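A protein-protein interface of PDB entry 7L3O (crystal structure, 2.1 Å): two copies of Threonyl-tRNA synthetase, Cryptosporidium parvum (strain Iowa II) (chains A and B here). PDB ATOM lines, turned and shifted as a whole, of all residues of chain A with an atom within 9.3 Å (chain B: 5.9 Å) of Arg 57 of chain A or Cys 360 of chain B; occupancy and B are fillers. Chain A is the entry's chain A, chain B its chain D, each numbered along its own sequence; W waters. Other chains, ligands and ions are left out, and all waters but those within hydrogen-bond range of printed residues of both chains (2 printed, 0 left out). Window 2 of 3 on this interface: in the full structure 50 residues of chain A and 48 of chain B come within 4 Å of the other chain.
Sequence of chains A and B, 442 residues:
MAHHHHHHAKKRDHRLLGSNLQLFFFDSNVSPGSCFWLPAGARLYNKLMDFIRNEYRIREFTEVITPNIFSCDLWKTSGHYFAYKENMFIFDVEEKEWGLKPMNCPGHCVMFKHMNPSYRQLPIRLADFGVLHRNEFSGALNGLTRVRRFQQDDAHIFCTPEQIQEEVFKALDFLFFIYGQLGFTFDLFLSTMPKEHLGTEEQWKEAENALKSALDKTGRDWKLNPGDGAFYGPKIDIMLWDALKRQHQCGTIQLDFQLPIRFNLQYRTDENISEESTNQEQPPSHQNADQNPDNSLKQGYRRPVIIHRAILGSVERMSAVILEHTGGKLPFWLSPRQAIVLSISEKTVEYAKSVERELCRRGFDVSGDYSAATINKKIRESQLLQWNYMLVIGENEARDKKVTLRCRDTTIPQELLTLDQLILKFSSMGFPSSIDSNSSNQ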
ATOM      1  N   MET A  49      31.462  -8.030   7.513  1.00  0.00           N
ATOM      2  CA  MET A  49      31.414  -9.484   7.552  1.00  0.00           C
ATOM      3  C   MET A  49      31.021 -10.002   8.939  1.00  0.00           C
ATOM      4  O   MET A  49      30.277 -10.983   9.048  1.00  0.00           O
ATOM      5  CB  MET A  49      32.770 -10.066   7.148  1.00  0.00           C
ATOM      6  CG  MET A  49      33.173  -9.808   5.718  1.00  0.00           C
ATOM      7  SD  MET A  49      34.648 -10.739   5.306  1.00  0.00           S
ATOM      8  CE  MET A  49      35.838 -10.016   6.401  1.00  0.00           C
ATOM      9  N   ASP A  50      31.541  -9.384  10.011  1.00  0.00           N
ATOM     10  CA  ASP A  50      31.211  -9.852  11.353  1.00  0.00           C
ATOM     11  C   ASP A  50      29.720  -9.742  11.625  1.00  0.00           C
ATOM     12  O   ASP A  50      29.141 -10.615  12.277  1.00  0.00           O
ATOM     13  CB  ASP A  50      31.973  -9.063  12.413  1.00  0.00           C
ATOM     14  CG  ASP A  50      33.451  -9.456  12.505  1.00  0.00           C
ATOM     15  OD1 ASP A  50      33.835 -10.529  11.985  1.00  0.00           O
ATOM     16  OD2 ASP A  50      34.224  -8.672  13.099  1.00  0.00           O
ATOM     17  N   PHE A  51      29.104  -8.649  11.180  1.00  0.00           N
ATOM     18  CA  PHE A  51      27.657  -8.479  11.264  1.00  0.00           C
ATOM     19  C   PHE A  51      26.922  -9.693  10.682  1.00  0.00           C
ATOM     20  O   PHE A  51      26.103 -10.332  11.350  1.00  0.00           O
ATOM     21  CB  PHE A  51      27.289  -7.190  10.520  1.00  0.00           C
ATOM     22  CG  PHE A  51      25.820  -6.835  10.561  1.00  0.00           C
ATOM     23  CD1 PHE A  51      25.010  -7.241  11.606  1.00  0.00           C
ATOM     24  CD2 PHE A  51      25.271  -6.060   9.556  1.00  0.00           C
ATOM     25  CE1 PHE A  51      23.669  -6.905  11.638  1.00  0.00           C
ATOM     26  CE2 PHE A  51      23.925  -5.713   9.571  1.00  0.00           C
ATOM     27  CZ  PHE A  51      23.123  -6.132  10.625  1.00  0.00           C
ATOM     28  N   ILE A  52      27.227 -10.025   9.429  1.00  0.00           N
ATOM     29  CA  ILE A  52      26.640 -11.191   8.770  1.00  0.00           C
ATOM     30  C   ILE A  52      26.959 -12.470   9.543  1.00  0.00           C
ATOM     31  O   ILE A  52      26.082 -13.321   9.771  1.00  0.00           O
ATOM     32  CB  ILE A  52      27.152 -11.259   7.317  1.00  0.00           C
ATOM     33  CG1 ILE A  52      26.627 -10.050   6.513  1.00  0.00           C
ATOM     34  CG2 ILE A  52      26.812 -12.608   6.656  1.00  0.00           C
ATOM     35  CD1 ILE A  52      25.136 -10.112   6.203  1.00  0.00           C
ATOM     36  N   ARG A  53      28.217 -12.621   9.971  1.00  0.00           N
ATOM     37  CA  ARG A  53      28.613 -13.852  10.644  1.00  0.00           C
ATOM     38  C   ARG A  53      27.786 -14.077  11.893  1.00  0.00           C
ATOM     39  O   ARG A  53      27.394 -15.211  12.190  1.00  0.00           O
ATOM     40  CB  ARG A  53      30.109 -13.813  11.003  1.00  0.00           C
ATOM     41  CG  ARG A  53      31.038 -14.082   9.825  1.00  0.00           C
ATOM     42  CD  ARG A  53      32.504 -14.149  10.266  1.00  0.00           C
ATOM     43  NE  ARG A  53      33.368 -14.519   9.155  1.00  0.00           N
ATOM     44  CZ  ARG A  53      34.393 -13.798   8.721  1.00  0.00           C
ATOM     45  NH1 ARG A  53      34.754 -12.674   9.320  1.00  0.00           N
ATOM     46  NH2 ARG A  53      35.088 -14.228   7.672  1.00  0.00           N
ATOM     47  N   ASN A  54      27.533 -13.010  12.649  1.00  0.00           N
ATOM     48  CA  ASN A  54      26.682 -13.109  13.829  1.00  0.00           C
ATOM     49  C   ASN A  54      25.310 -13.650  13.447  1.00  0.00           C
ATOM     50  O   ASN A  54      24.758 -14.518  14.125  1.00  0.00           O
ATOM     51  CB  ASN A  54      26.569 -11.729  14.489  1.00  0.00           C
ATOM     52  CG  ASN A  54      25.989 -11.781  15.894  1.00  0.00           C
ATOM     53  OD1 ASN A  54      26.569 -12.389  16.793  1.00  0.00           O
ATOM     54  ND2 ASN A  54      24.842 -11.113  16.095  1.00  0.00           N
ATOM     55  N   GLU A  55      24.757 -13.173  12.338  1.00  0.00           N
ATOM     56  CA  GLU A  55      23.473 -13.722  11.919  1.00  0.00           C
ATOM     57  C   GLU A  55      23.609 -15.155  11.434  1.00  0.00           C
ATOM     58  O   GLU A  55      22.686 -15.945  11.637  1.00  0.00           O
ATOM     59  CB  GLU A  55      22.840 -12.845  10.853  1.00  0.00           C
ATOM     60  CG  GLU A  55      22.356 -11.516  11.410  1.00  0.00           C
ATOM     61  CD  GLU A  55      21.191 -11.667  12.377  1.00  0.00           C
ATOM     62  OE1 GLU A  55      20.160 -12.288  12.009  1.00  0.00           O
ATOM     63  OE2 GLU A  55      21.298 -11.157  13.509  1.00  0.00           O
ATOM     64  N   TYR A  56      24.747 -15.523  10.825  1.00  0.00           N
ATOM     65  CA  TYR A  56      24.943 -16.926  10.460  1.00  0.00           C
ATOM     66  C   TYR A  56      24.804 -17.822  11.675  1.00  0.00           C
ATOM     67  O   TYR A  56      24.129 -18.855  11.616  1.00  0.00           O
ATOM     68  CB  TYR A  56      26.312 -17.148   9.806  1.00  0.00           C
ATOM     69  CG  TYR A  56      26.400 -16.671   8.371  1.00  0.00           C
ATOM     70  CD1 TYR A  56      25.242 -16.474   7.601  1.00  0.00           C
ATOM     71  CD2 TYR A  56      27.631 -16.437   7.772  1.00  0.00           C
ATOM     72  CE1 TYR A  56      25.321 -16.041   6.286  1.00  0.00           C
ATOM     73  CE2 TYR A  56      27.723 -16.023   6.459  1.00  0.00           C
ATOM     74  CZ  TYR A  56      26.564 -15.812   5.719  1.00  0.00           C
ATOM     75  OH  TYR A  56      26.665 -15.384   4.409  1.00  0.00           O
ATOM     76  N   ARG A  57      25.427 -17.438  12.795  1.00  0.00           N
ATOM     77  CA  ARG A  57      25.316 -18.239  14.004  1.00  0.00           C
ATOM     78  C   ARG A  57      23.866 -18.320  14.469  1.00  0.00           C
ATOM     79  O   ARG A  57      23.367 -19.400  14.783  1.00  0.00           O
ATOM     80  CB  ARG A  57      26.209 -17.664  15.111  1.00  0.00           C
ATOM     81  CG  ARG A  57      27.713 -17.592  14.772  1.00  0.00           C
ATOM     82  CD  ARG A  57      28.527 -17.185  16.021  1.00  0.00           C
ATOM     83  NE  ARG A  57      27.974 -17.872  17.181  1.00  0.00           N
ATOM     84  CZ  ARG A  57      28.433 -19.019  17.670  1.00  0.00           C
ATOM     85  NH1 ARG A  57      29.571 -19.555  17.233  1.00  0.00           N
ATOM     86  NH2 ARG A  57      27.718 -19.658  18.603  1.00  0.00           N
ATOM     87  N   ILE A  58      23.175 -17.181  14.531  1.00  0.00           N
ATOM     88  CA  ILE A  58      21.763 -17.195  14.927  1.00  0.00           C
ATOM     89  C   ILE A  58      20.942 -18.072  13.986  1.00  0.00           C
ATOM     90  O   ILE A  58      20.008 -18.758  14.415  1.00  0.00           O
ATOM     91  CB  ILE A  58      21.202 -15.753  14.984  1.00  0.00           C
ATOM     92  CG1 ILE A  58      21.819 -14.968  16.151  1.00  0.00           C
ATOM     93  CG2 ILE A  58      19.681 -15.748  15.096  1.00  0.00           C
ATOM     94  CD1 ILE A  58      21.619 -13.462  16.053  1.00  0.00           C
ATOM     95  N   ARG A  59      21.287 -18.091  12.702  1.00  0.00           N
ATOM     96  CA  ARG A  59      20.437 -18.726  11.705  1.00  0.00           C
ATOM     97  C   ARG A  59      21.018 -20.036  11.190  1.00  0.00           C
ATOM     98  O   ARG A  59      20.536 -20.551  10.181  1.00  0.00           O
ATOM     99  CB  ARG A  59      20.169 -17.758  10.546  1.00  0.00           C
ATOM    100  CG  ARG A  59      19.612 -16.416  10.984  1.00  0.00           C
ATOM    101  CD  ARG A  59      19.533 -15.413   9.834  1.00  0.00           C
ATOM    102  NE  ARG A  59      19.004 -14.126  10.288  1.00  0.00           N
ATOM    103  CZ  ARG A  59      17.752 -13.712  10.124  1.00  0.00           C
ATOM    104  NH1 ARG A  59      16.846 -14.455   9.492  1.00  0.00           N
ATOM    105  NH2 ARG A  59      17.395 -12.521  10.602  1.00  0.00           N
ATOM    106  N   GLU A  60      22.037 -20.584  11.860  1.00  0.00           N
ATOM    107  CA  GLU A  60      22.536 -21.945  11.601  1.00  0.00           C
ATOM    108  C   GLU A  60      23.058 -22.114  10.171  1.00  0.00           C
ATOM    109  O   GLU A  60      22.724 -23.072   9.464  1.00  0.00           O
ATOM    110  CB  GLU A  60      21.459 -22.986  11.936  1.00  0.00           C
ATOM    111  CG  GLU A  60      21.048 -22.939  13.423  1.00  0.00           C
ATOM    112  CD  GLU A  60      20.250 -24.148  13.875  1.00  0.00           C
ATOM    113  OE1 GLU A  60      19.146 -24.367  13.341  1.00  0.00           O
ATOM    114  OE2 GLU A  60      20.740 -24.888  14.757  1.00  0.00           O
ATOM    115  N   PHE A  61      23.865 -21.145   9.744  1.00  0.00           N
ATOM    116  CA  PHE A  61      24.756 -21.254   8.598  1.00  0.00           C
ATOM    117  C   PHE A  61      26.150 -21.599   9.110  1.00  0.00           C
ATOM    118  O   PHE A  61      26.581 -21.084  10.146  1.00  0.00           O
ATOM    119  CB  PHE A  61      24.842 -19.940   7.818  1.00  0.00           C
ATOM    120  CG  PHE A  61      23.659 -19.645   6.929  1.00  0.00           C
ATOM    121  CD1 PHE A  61      22.432 -19.283   7.466  1.00  0.00           C
ATOM    122  CD2 PHE A  61      23.802 -19.655   5.549  1.00  0.00           C
ATOM    123  CE1 PHE A  61      21.342 -18.975   6.634  1.00  0.00           C
ATOM    124  CE2 PHE A  61      22.718 -19.334   4.702  1.00  0.00           C
ATOM    125  CZ  PHE A  61      21.492 -19.006   5.253  1.00  0.00           C
ATOM    126  N   THR A  62      26.864 -22.446   8.374  1.00  0.00           N
ATOM    127  CA  THR A  62      28.208 -22.858   8.761  1.00  0.00           C
ATOM    128  C   THR A  62      29.184 -22.354   7.717  1.00  0.00           C
ATOM    129  O   THR A  62      29.133 -22.779   6.560  1.00  0.00           O
ATOM    130  CB  THR A  62      28.317 -24.374   8.898  1.00  0.00           C
ATOM    131  OG1 THR A  62      27.941 -24.987   7.658  1.00  0.00           O
ATOM    132  CG2 THR A  62      27.385 -24.876   9.991  1.00  0.00           C
ATOM    133  N   GLU A  63      30.080 -21.468   8.130  1.00  0.00           N
ATOM    134  CA  GLU A  63      31.109 -20.987   7.221  1.00  0.00           C
ATOM    135  C   GLU A  63      32.107 -22.089   6.882  1.00  0.00           C
ATOM    136  O   GLU A  63      32.474 -22.909   7.739  1.00  0.00           O
ATOM    137  CB  GLU A  63      31.825 -19.806   7.846  1.00  0.00           C
ATOM    138  CG  GLU A  63      32.658 -19.037   6.881  1.00  0.00           C
ATOM    139  CD  GLU A  63      33.144 -17.737   7.471  1.00  0.00           C
ATOM    140  OE1 GLU A  63      32.483 -17.222   8.407  1.00  0.00           O
ATOM    141  OE2 GLU A  63      34.181 -17.236   6.996  1.00  0.00           O
ATOM    142  N   ARG A 125      23.875 -25.683   5.128  1.00  0.00           N
ATOM    143  CA  ARG A 125      24.011 -24.275   4.757  1.00  0.00           C
ATOM    144  C   ARG A 125      25.486 -23.900   4.804  1.00  0.00           C
ATOM    145  O   ARG A 125      26.008 -23.517   5.856  1.00  0.00           O
ATOM    146  CB  ARG A 125      23.161 -23.385   5.669  1.00  0.00           C
ATOM    147  CG  ARG A 125      21.683 -23.779   5.686  1.00  0.00           C
ATOM    148  CD  ARG A 125      20.841 -22.803   6.474  1.00  0.00           C
ATOM    149  NE  ARG A 125      19.494 -23.317   6.700  1.00  0.00           N
ATOM    150  CZ  ARG A 125      19.144 -24.044   7.756  1.00  0.00           C
ATOM    151  NH1 ARG A 125      20.016 -24.347   8.713  1.00  0.00           N
ATOM    152  NH2 ARG A 125      17.894 -24.498   7.851  1.00  0.00           N
ATOM    153  N   ALA A 127      28.324 -21.401   4.047  1.00  0.00           N
ATOM    154  CA  ALA A 127      28.606 -20.002   3.765  1.00  0.00           C
ATOM    155  C   ALA A 127      30.091 -19.841   3.486  1.00  0.00           C
ATOM    156  O   ALA A 127      30.928 -20.528   4.079  1.00  0.00           O
ATOM    157  CB  ALA A 127      28.188 -19.095   4.923  1.00  0.00           C
ATOM    158  N   PHE A 174      15.908 -13.197   6.337  1.00  0.00           N
ATOM    159  CA  PHE A 174      17.295 -12.778   6.576  1.00  0.00           C
ATOM    160  C   PHE A 174      17.580 -11.466   5.849  1.00  0.00           C
ATOM    161  O   PHE A 174      18.062 -10.494   6.445  1.00  0.00           O
ATOM    162  CB  PHE A 174      18.233 -13.908   6.106  1.00  0.00           C
ATOM    163  CG  PHE A 174      19.675 -13.843   6.623  1.00  0.00           C
ATOM    164  CD1 PHE A 174      20.179 -12.728   7.268  1.00  0.00           C
ATOM    165  CD2 PHE A 174      20.526 -14.930   6.415  1.00  0.00           C
ATOM    166  CE1 PHE A 174      21.521 -12.703   7.712  1.00  0.00           C
ATOM    167  CE2 PHE A 174      21.867 -14.915   6.864  1.00  0.00           C
ATOM    168  CZ  PHE A 174      22.347 -13.793   7.499  1.00  0.00           C
ATOM    169  N   SER A 433      20.885  -7.209  16.296  1.00  0.00           N
ATOM    170  CA  SER A 433      20.687  -8.644  16.384  1.00  0.00           C
ATOM    171  C   SER A 433      19.232  -8.969  16.088  1.00  0.00           C
ATOM    172  O   SER A 433      18.330  -8.248  16.526  1.00  0.00           O
ATOM    173  CB  SER A 433      21.060  -9.156  17.778  1.00  0.00           C
ATOM    174  OG  SER A 433      21.053 -10.565  17.818  1.00  0.00           O
ATOM    175  N   SER A 434      19.002 -10.059  15.355  1.00  0.00           N
ATOM    176  CA  SER A 434      17.637 -10.475  15.055  1.00  0.00           C
ATOM    177  C   SER A 434      16.945 -11.136  16.237  1.00  0.00           C
ATOM    178  O   SER A 434      15.774 -11.496  16.121  1.00  0.00           O
ATOM    179  CB  SER A 434      17.615 -11.416  13.846  1.00  0.00           C
ATOM    180  OG  SER A 434      18.317 -12.619  14.092  1.00  0.00           O
ATOM    181  N   ILE A 435      17.638 -11.313  17.361  1.00  0.00           N
ATOM    182  CA  ILE A 435      17.024 -11.790  18.593  1.00  0.00           C
ATOM    183  C   ILE A 435      16.993 -10.722  19.673  1.00  0.00           C
ATOM    184  O   ILE A 435      16.453 -10.972  20.760  1.00  0.00           O
ATOM    185  CB  ILE A 435      17.733 -13.056  19.109  1.00  0.00           C
ATOM    186  CG1 ILE A 435      19.235 -12.806  19.222  1.00  0.00           C
ATOM    187  CG2 ILE A 435      17.449 -14.236  18.186  1.00  0.00           C
ATOM    188  CD1 ILE A 435      20.037 -14.044  19.548  1.00  0.00           C
ATOM    189  N   VAL B 355      18.920 -25.132  26.505  1.00  0.00           N
ATOM    190  CA  VAL B 355      20.284 -24.893  26.959  1.00  0.00           C
ATOM    191  C   VAL B 355      21.215 -24.747  25.763  1.00  0.00           C
ATOM    192  O   VAL B 355      22.003 -23.801  25.688  1.00  0.00           O
ATOM    193  CB  VAL B 355      20.746 -26.016  27.905  1.00  0.00           C
ATOM    194  CG1 VAL B 355      22.253 -25.959  28.097  1.00  0.00           C
ATOM    195  CG2 VAL B 355      20.035 -25.913  29.252  1.00  0.00           C
ATOM    196  N   GLU B 356      21.130 -25.677  24.806  1.00  0.00           N
ATOM    197  CA  GLU B 356      21.982 -25.590  23.625  1.00  0.00           C
ATOM    198  C   GLU B 356      21.748 -24.287  22.874  1.00  0.00           C
ATOM    199  O   GLU B 356      22.701 -23.655  22.397  1.00  0.00           O
ATOM    200  CB  GLU B 356      21.746 -26.782  22.700  1.00  0.00           C
ATOM    201  CG  GLU B 356      22.740 -26.817  21.531  1.00  0.00           C
ATOM    202  CD  GLU B 356      22.253 -27.604  20.317  1.00  0.00           C
ATOM    203  OE1 GLU B 356      21.324 -28.434  20.441  1.00  0.00           O
ATOM    204  OE2 GLU B 356      22.811 -27.386  19.224  1.00  0.00           O
ATOM    205  N   ARG B 357      20.485 -23.857  22.776  1.00  0.00           N
ATOM    206  CA  ARG B 357      20.160 -22.640  22.033  1.00  0.00           C
ATOM    207  C   ARG B 357      20.811 -21.414  22.658  1.00  0.00           C
ATOM    208  O   ARG B 357      21.433 -20.605  21.963  1.00  0.00           O
ATOM    209  CB  ARG B 357      18.643 -22.450  21.955  1.00  0.00           C
ATOM    210  CG  ARG B 357      18.077 -22.833  20.609  1.00  0.00           C
ATOM    211  CD  ARG B 357      16.625 -22.438  20.458  1.00  0.00           C
ATOM    212  NE  ARG B 357      15.751 -23.599  20.331  1.00  0.00           N
ATOM    213  CZ  ARG B 357      15.025 -24.102  21.322  1.00  0.00           C
ATOM    214  NH1 ARG B 357      15.066 -23.585  22.540  1.00  0.00           N
ATOM    215  NH2 ARG B 357      14.223 -25.137  21.080  1.00  0.00           N
ATOM    216  N   GLU B 358      20.664 -21.249  23.970  1.00  0.00           N
ATOM    217  CA  GLU B 358      21.244 -20.078  24.614  1.00  0.00           C
ATOM    218  C   GLU B 358      22.764 -20.087  24.486  1.00  0.00           C
ATOM    219  O   GLU B 358      23.377 -19.048  24.215  1.00  0.00           O
ATOM    220  CB  GLU B 358      20.807 -20.023  26.076  1.00  0.00           C
ATOM    221  CG  GLU B 358      21.327 -18.830  26.857  1.00  0.00           C
ATOM    222  CD  GLU B 358      20.796 -17.500  26.356  1.00  0.00           C
ATOM    223  OE1 GLU B 358      19.648 -17.444  25.850  1.00  0.00           O
ATOM    224  OE2 GLU B 358      21.540 -16.502  26.481  1.00  0.00           O
ATOM    225  N   LEU B 359      23.386 -21.256  24.646  1.00  0.00           N
ATOM    226  CA  LEU B 359      24.829 -21.340  24.463  1.00  0.00           C
ATOM    227  C   LEU B 359      25.226 -20.930  23.057  1.00  0.00           C
ATOM    228  O   LEU B 359      26.224 -20.222  22.870  1.00  0.00           O
ATOM    229  CB  LEU B 359      25.321 -22.754  24.760  1.00  0.00           C
ATOM    230  CG  LEU B 359      25.281 -23.170  26.228  1.00  0.00           C
ATOM    231  CD1 LEU B 359      25.671 -24.619  26.339  1.00  0.00           C
ATOM    232  CD2 LEU B 359      26.195 -22.296  27.085  1.00  0.00           C
ATOM    233  N   CYS B 360      24.452 -21.359  22.052  1.00  0.00           N
ATOM    234  CA  CYS B 360      24.731 -20.936  20.687  1.00  0.00           C
ATOM    235  C   CYS B 360      24.608 -19.427  20.555  1.00  0.00           C
ATOM    236  O   CYS B 360      25.475 -18.775  19.962  1.00  0.00           O
ATOM    237  CB  CYS B 360      23.793 -21.633  19.695  1.00  0.00           C
ATOM    238  SG  CYS B 360      24.153 -21.189  17.966  1.00  0.00           S
ATOM    239  N   ARG B 361      23.533 -18.853  21.114  1.00  0.00           N
ATOM    240  CA  ARG B 361      23.303 -17.413  21.024  1.00  0.00           C
ATOM    241  C   ARG B 361      24.403 -16.626  21.723  1.00  0.00           C
ATOM    242  O   ARG B 361      24.699 -15.490  21.336  1.00  0.00           O
ATOM    243  CB  ARG B 361      21.943 -17.049  21.628  1.00  0.00           C
ATOM    244  CG  ARG B 361      20.735 -17.631  20.908  1.00  0.00           C
ATOM    245  CD  ARG B 361      19.424 -17.208  21.572  1.00  0.00           C
ATOM    246  NE  ARG B 361      18.270 -17.715  20.836  1.00  0.00           N
ATOM    247  CZ  ARG B 361      17.016 -17.333  21.033  1.00  0.00           C
ATOM    248  NH1 ARG B 361      16.704 -16.416  21.936  1.00  0.00           N
ATOM    249  NH2 ARG B 361      16.047 -17.881  20.302  1.00  0.00           N
ATOM    250  N   ARG B 362      25.011 -17.204  22.752  1.00  0.00           N
ATOM    251  CA  ARG B 362      26.107 -16.561  23.465  1.00  0.00           C
ATOM    252  C   ARG B 362      27.445 -16.696  22.750  1.00  0.00           C
ATOM    253  O   ARG B 362      28.455 -16.202  23.262  1.00  0.00           O
ATOM    254  CB  ARG B 362      26.217 -17.138  24.878  1.00  0.00           C
ATOM    255  CG  ARG B 362      25.042 -16.805  25.787  1.00  0.00           C
ATOM    256  CD  ARG B 362      24.907 -15.314  26.031  1.00  0.00           C
ATOM    257  NE  ARG B 362      23.959 -15.041  27.104  1.00  0.00           N
ATOM    258  CZ  ARG B 362      24.293 -14.571  28.299  1.00  0.00           C
ATOM    259  NH1 ARG B 362      25.544 -14.249  28.591  1.00  0.00           N
ATOM    260  NH2 ARG B 362      23.346 -14.412  29.223  1.00  0.00           N
ATOM    261  N   GLY B 363      27.486 -17.362  21.600  1.00  0.00           N
ATOM    262  CA  GLY B 363      28.683 -17.429  20.793  1.00  0.00           C
ATOM    263  C   GLY B 363      29.532 -18.672  20.967  1.00  0.00           C
ATOM    264  O   GLY B 363      30.656 -18.700  20.462  1.00  0.00           O
ATOM    265  N   PHE B 364      29.039 -19.700  21.643  1.00  0.00           N
ATOM    266  CA  PHE B 364      29.853 -20.895  21.808  1.00  0.00           C
ATOM    267  C   PHE B 364      29.500 -21.926  20.741  1.00  0.00           C
ATOM    268  O   PHE B 364      28.418 -21.897  20.141  1.00  0.00           O
ATOM    269  CB  PHE B 364      29.687 -21.467  23.214  1.00  0.00           C
ATOM    270  CG  PHE B 364      29.976 -20.462  24.288  1.00  0.00           C
ATOM    271  CD1 PHE B 364      31.287 -20.048  24.532  1.00  0.00           C
ATOM    272  CD2 PHE B 364      28.943 -19.894  25.026  1.00  0.00           C
ATOM    273  CE1 PHE B 364      31.554 -19.086  25.494  1.00  0.00           C
ATOM    274  CE2 PHE B 364      29.210 -18.954  26.002  1.00  0.00           C
ATOM    275  CZ  PHE B 364      30.512 -18.539  26.232  1.00  0.00           C
ATOM    276  N   ASP B 365      30.456 -22.816  20.474  1.00  0.00           N
ATOM    277  CA  ASP B 365      30.321 -23.807  19.411  1.00  0.00           C
ATOM    278  C   ASP B 365      29.813 -25.084  20.060  1.00  0.00           C
ATOM    279  O   ASP B 365      30.570 -25.816  20.712  1.00  0.00           O
ATOM    280  CB  ASP B 365      31.640 -24.008  18.675  1.00  0.00           C
ATOM    281  CG  ASP B 365      32.037 -22.784  17.860  1.00  0.00           C
ATOM    282  OD1 ASP B 365      31.145 -22.179  17.238  1.00  0.00           O
ATOM    283  OD2 ASP B 365      33.231 -22.415  17.859  1.00  0.00           O
ATOM    284  N   VAL B 366      28.518 -25.341  19.883  1.00  0.00           N
ATOM    285  CA  VAL B 366      27.805 -26.366  20.623  1.00  0.00           C
ATOM    286  C   VAL B 366      27.024 -27.229  19.644  1.00  0.00           C
ATOM    287  O   VAL B 366      26.887 -26.908  18.468  1.00  0.00           O
ATOM    288  CB  VAL B 366      26.867 -25.758  21.685  1.00  0.00           C
ATOM    289  CG1 VAL B 366      27.672 -24.922  22.690  1.00  0.00           C
ATOM    290  CG2 VAL B 366      25.781 -24.913  21.015  1.00  0.00           C
HETATM  291  O   HOH W   1      24.850 -21.900  14.398  1.00  0.00           O
HETATM  292  O   HOH W   2      27.023 -21.358  16.573  1.00  0.00           O
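O of Cys 360 of chain B sits at hydrogen-bond distance from NH2 of Arg 57 of chain A, 2.8 Å away. The guanidinium group of Arg 57 of chain A sits at hydrogen-bond distance from the backbone carbonyl oxygen of Phe 364 of chain B (2.8 Å). The side-chain carboxylate of Asp 365 of chain B is in salt-bridge range of the guanidinium group of Arg 57 of chain A.
The backbone carbonyl oxygen (O) of Leu 359 of chain B lies within hydrogen-bond range of the backbone NH (N) of Phe 364 of chain B (3.1 Å).
Arg 57 of chain A touches Gly 363 of chain B (NH2 to C, 3.1 Å). Ile 435 of chain A touches Arg 361 of chain B (CD1 to CD, 3.8 Å).
Arg 57 of chain A touches just these residues of chain B: Cys 360, Gly 363, Phe 364 and Asp 365. Cys 360 of chain B touches just one residue of chain A: Arg 57. Gly 363 of chain B touches just one residue of chain A: Arg 57 (3.1 Å). Of the printed residues of chain A, Phe 364 of chain B touches Arg 57 (2.8 Å). Of the printed residues of chain A, Arg 361 of chain B touches Ile 435. The nearest residue of chain B that does not touch Arg 57 of chain A is Leu 359 of chain B (4.6 Å). The nearest printed residue of chain A that does not touch Arg 361 of chain B is Arg 57 of chain A (4.9 Å).
Of the 21 printed residues of chain A, 2 touch a printed residue of chain B. Hydrophobic or aromatic side chains of chain A that line the printed part of chain B: Ile 435. Of the 12 printed residues of chain B, 5 touch a printed residue of chain A. Among the printed residues, 5 pairs touch across the chains. Among the printed residues, Asp or Glu carboxylates within 4 Å of a Lys or Arg side-chain nitrogen of the other chain: Arg 57 of chain A with Asp 365 of chain B.
No position is printed for both chains. Of the 5 pairs that touch across the chains among the printed residues, none has its exchanged pair printed and touching as well.
Water W2 bridges the guanidinium group (NH2) of Arg 57 of chain A and the side-chain sulfur (SG) of Cys 360 of chain B. Water W1 bridges the backbone carbonyl oxygen of Arg 57 of chain A (2.9 Å) and the side-chain sulfur of Cys 360 of chain B (3.7 Å).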
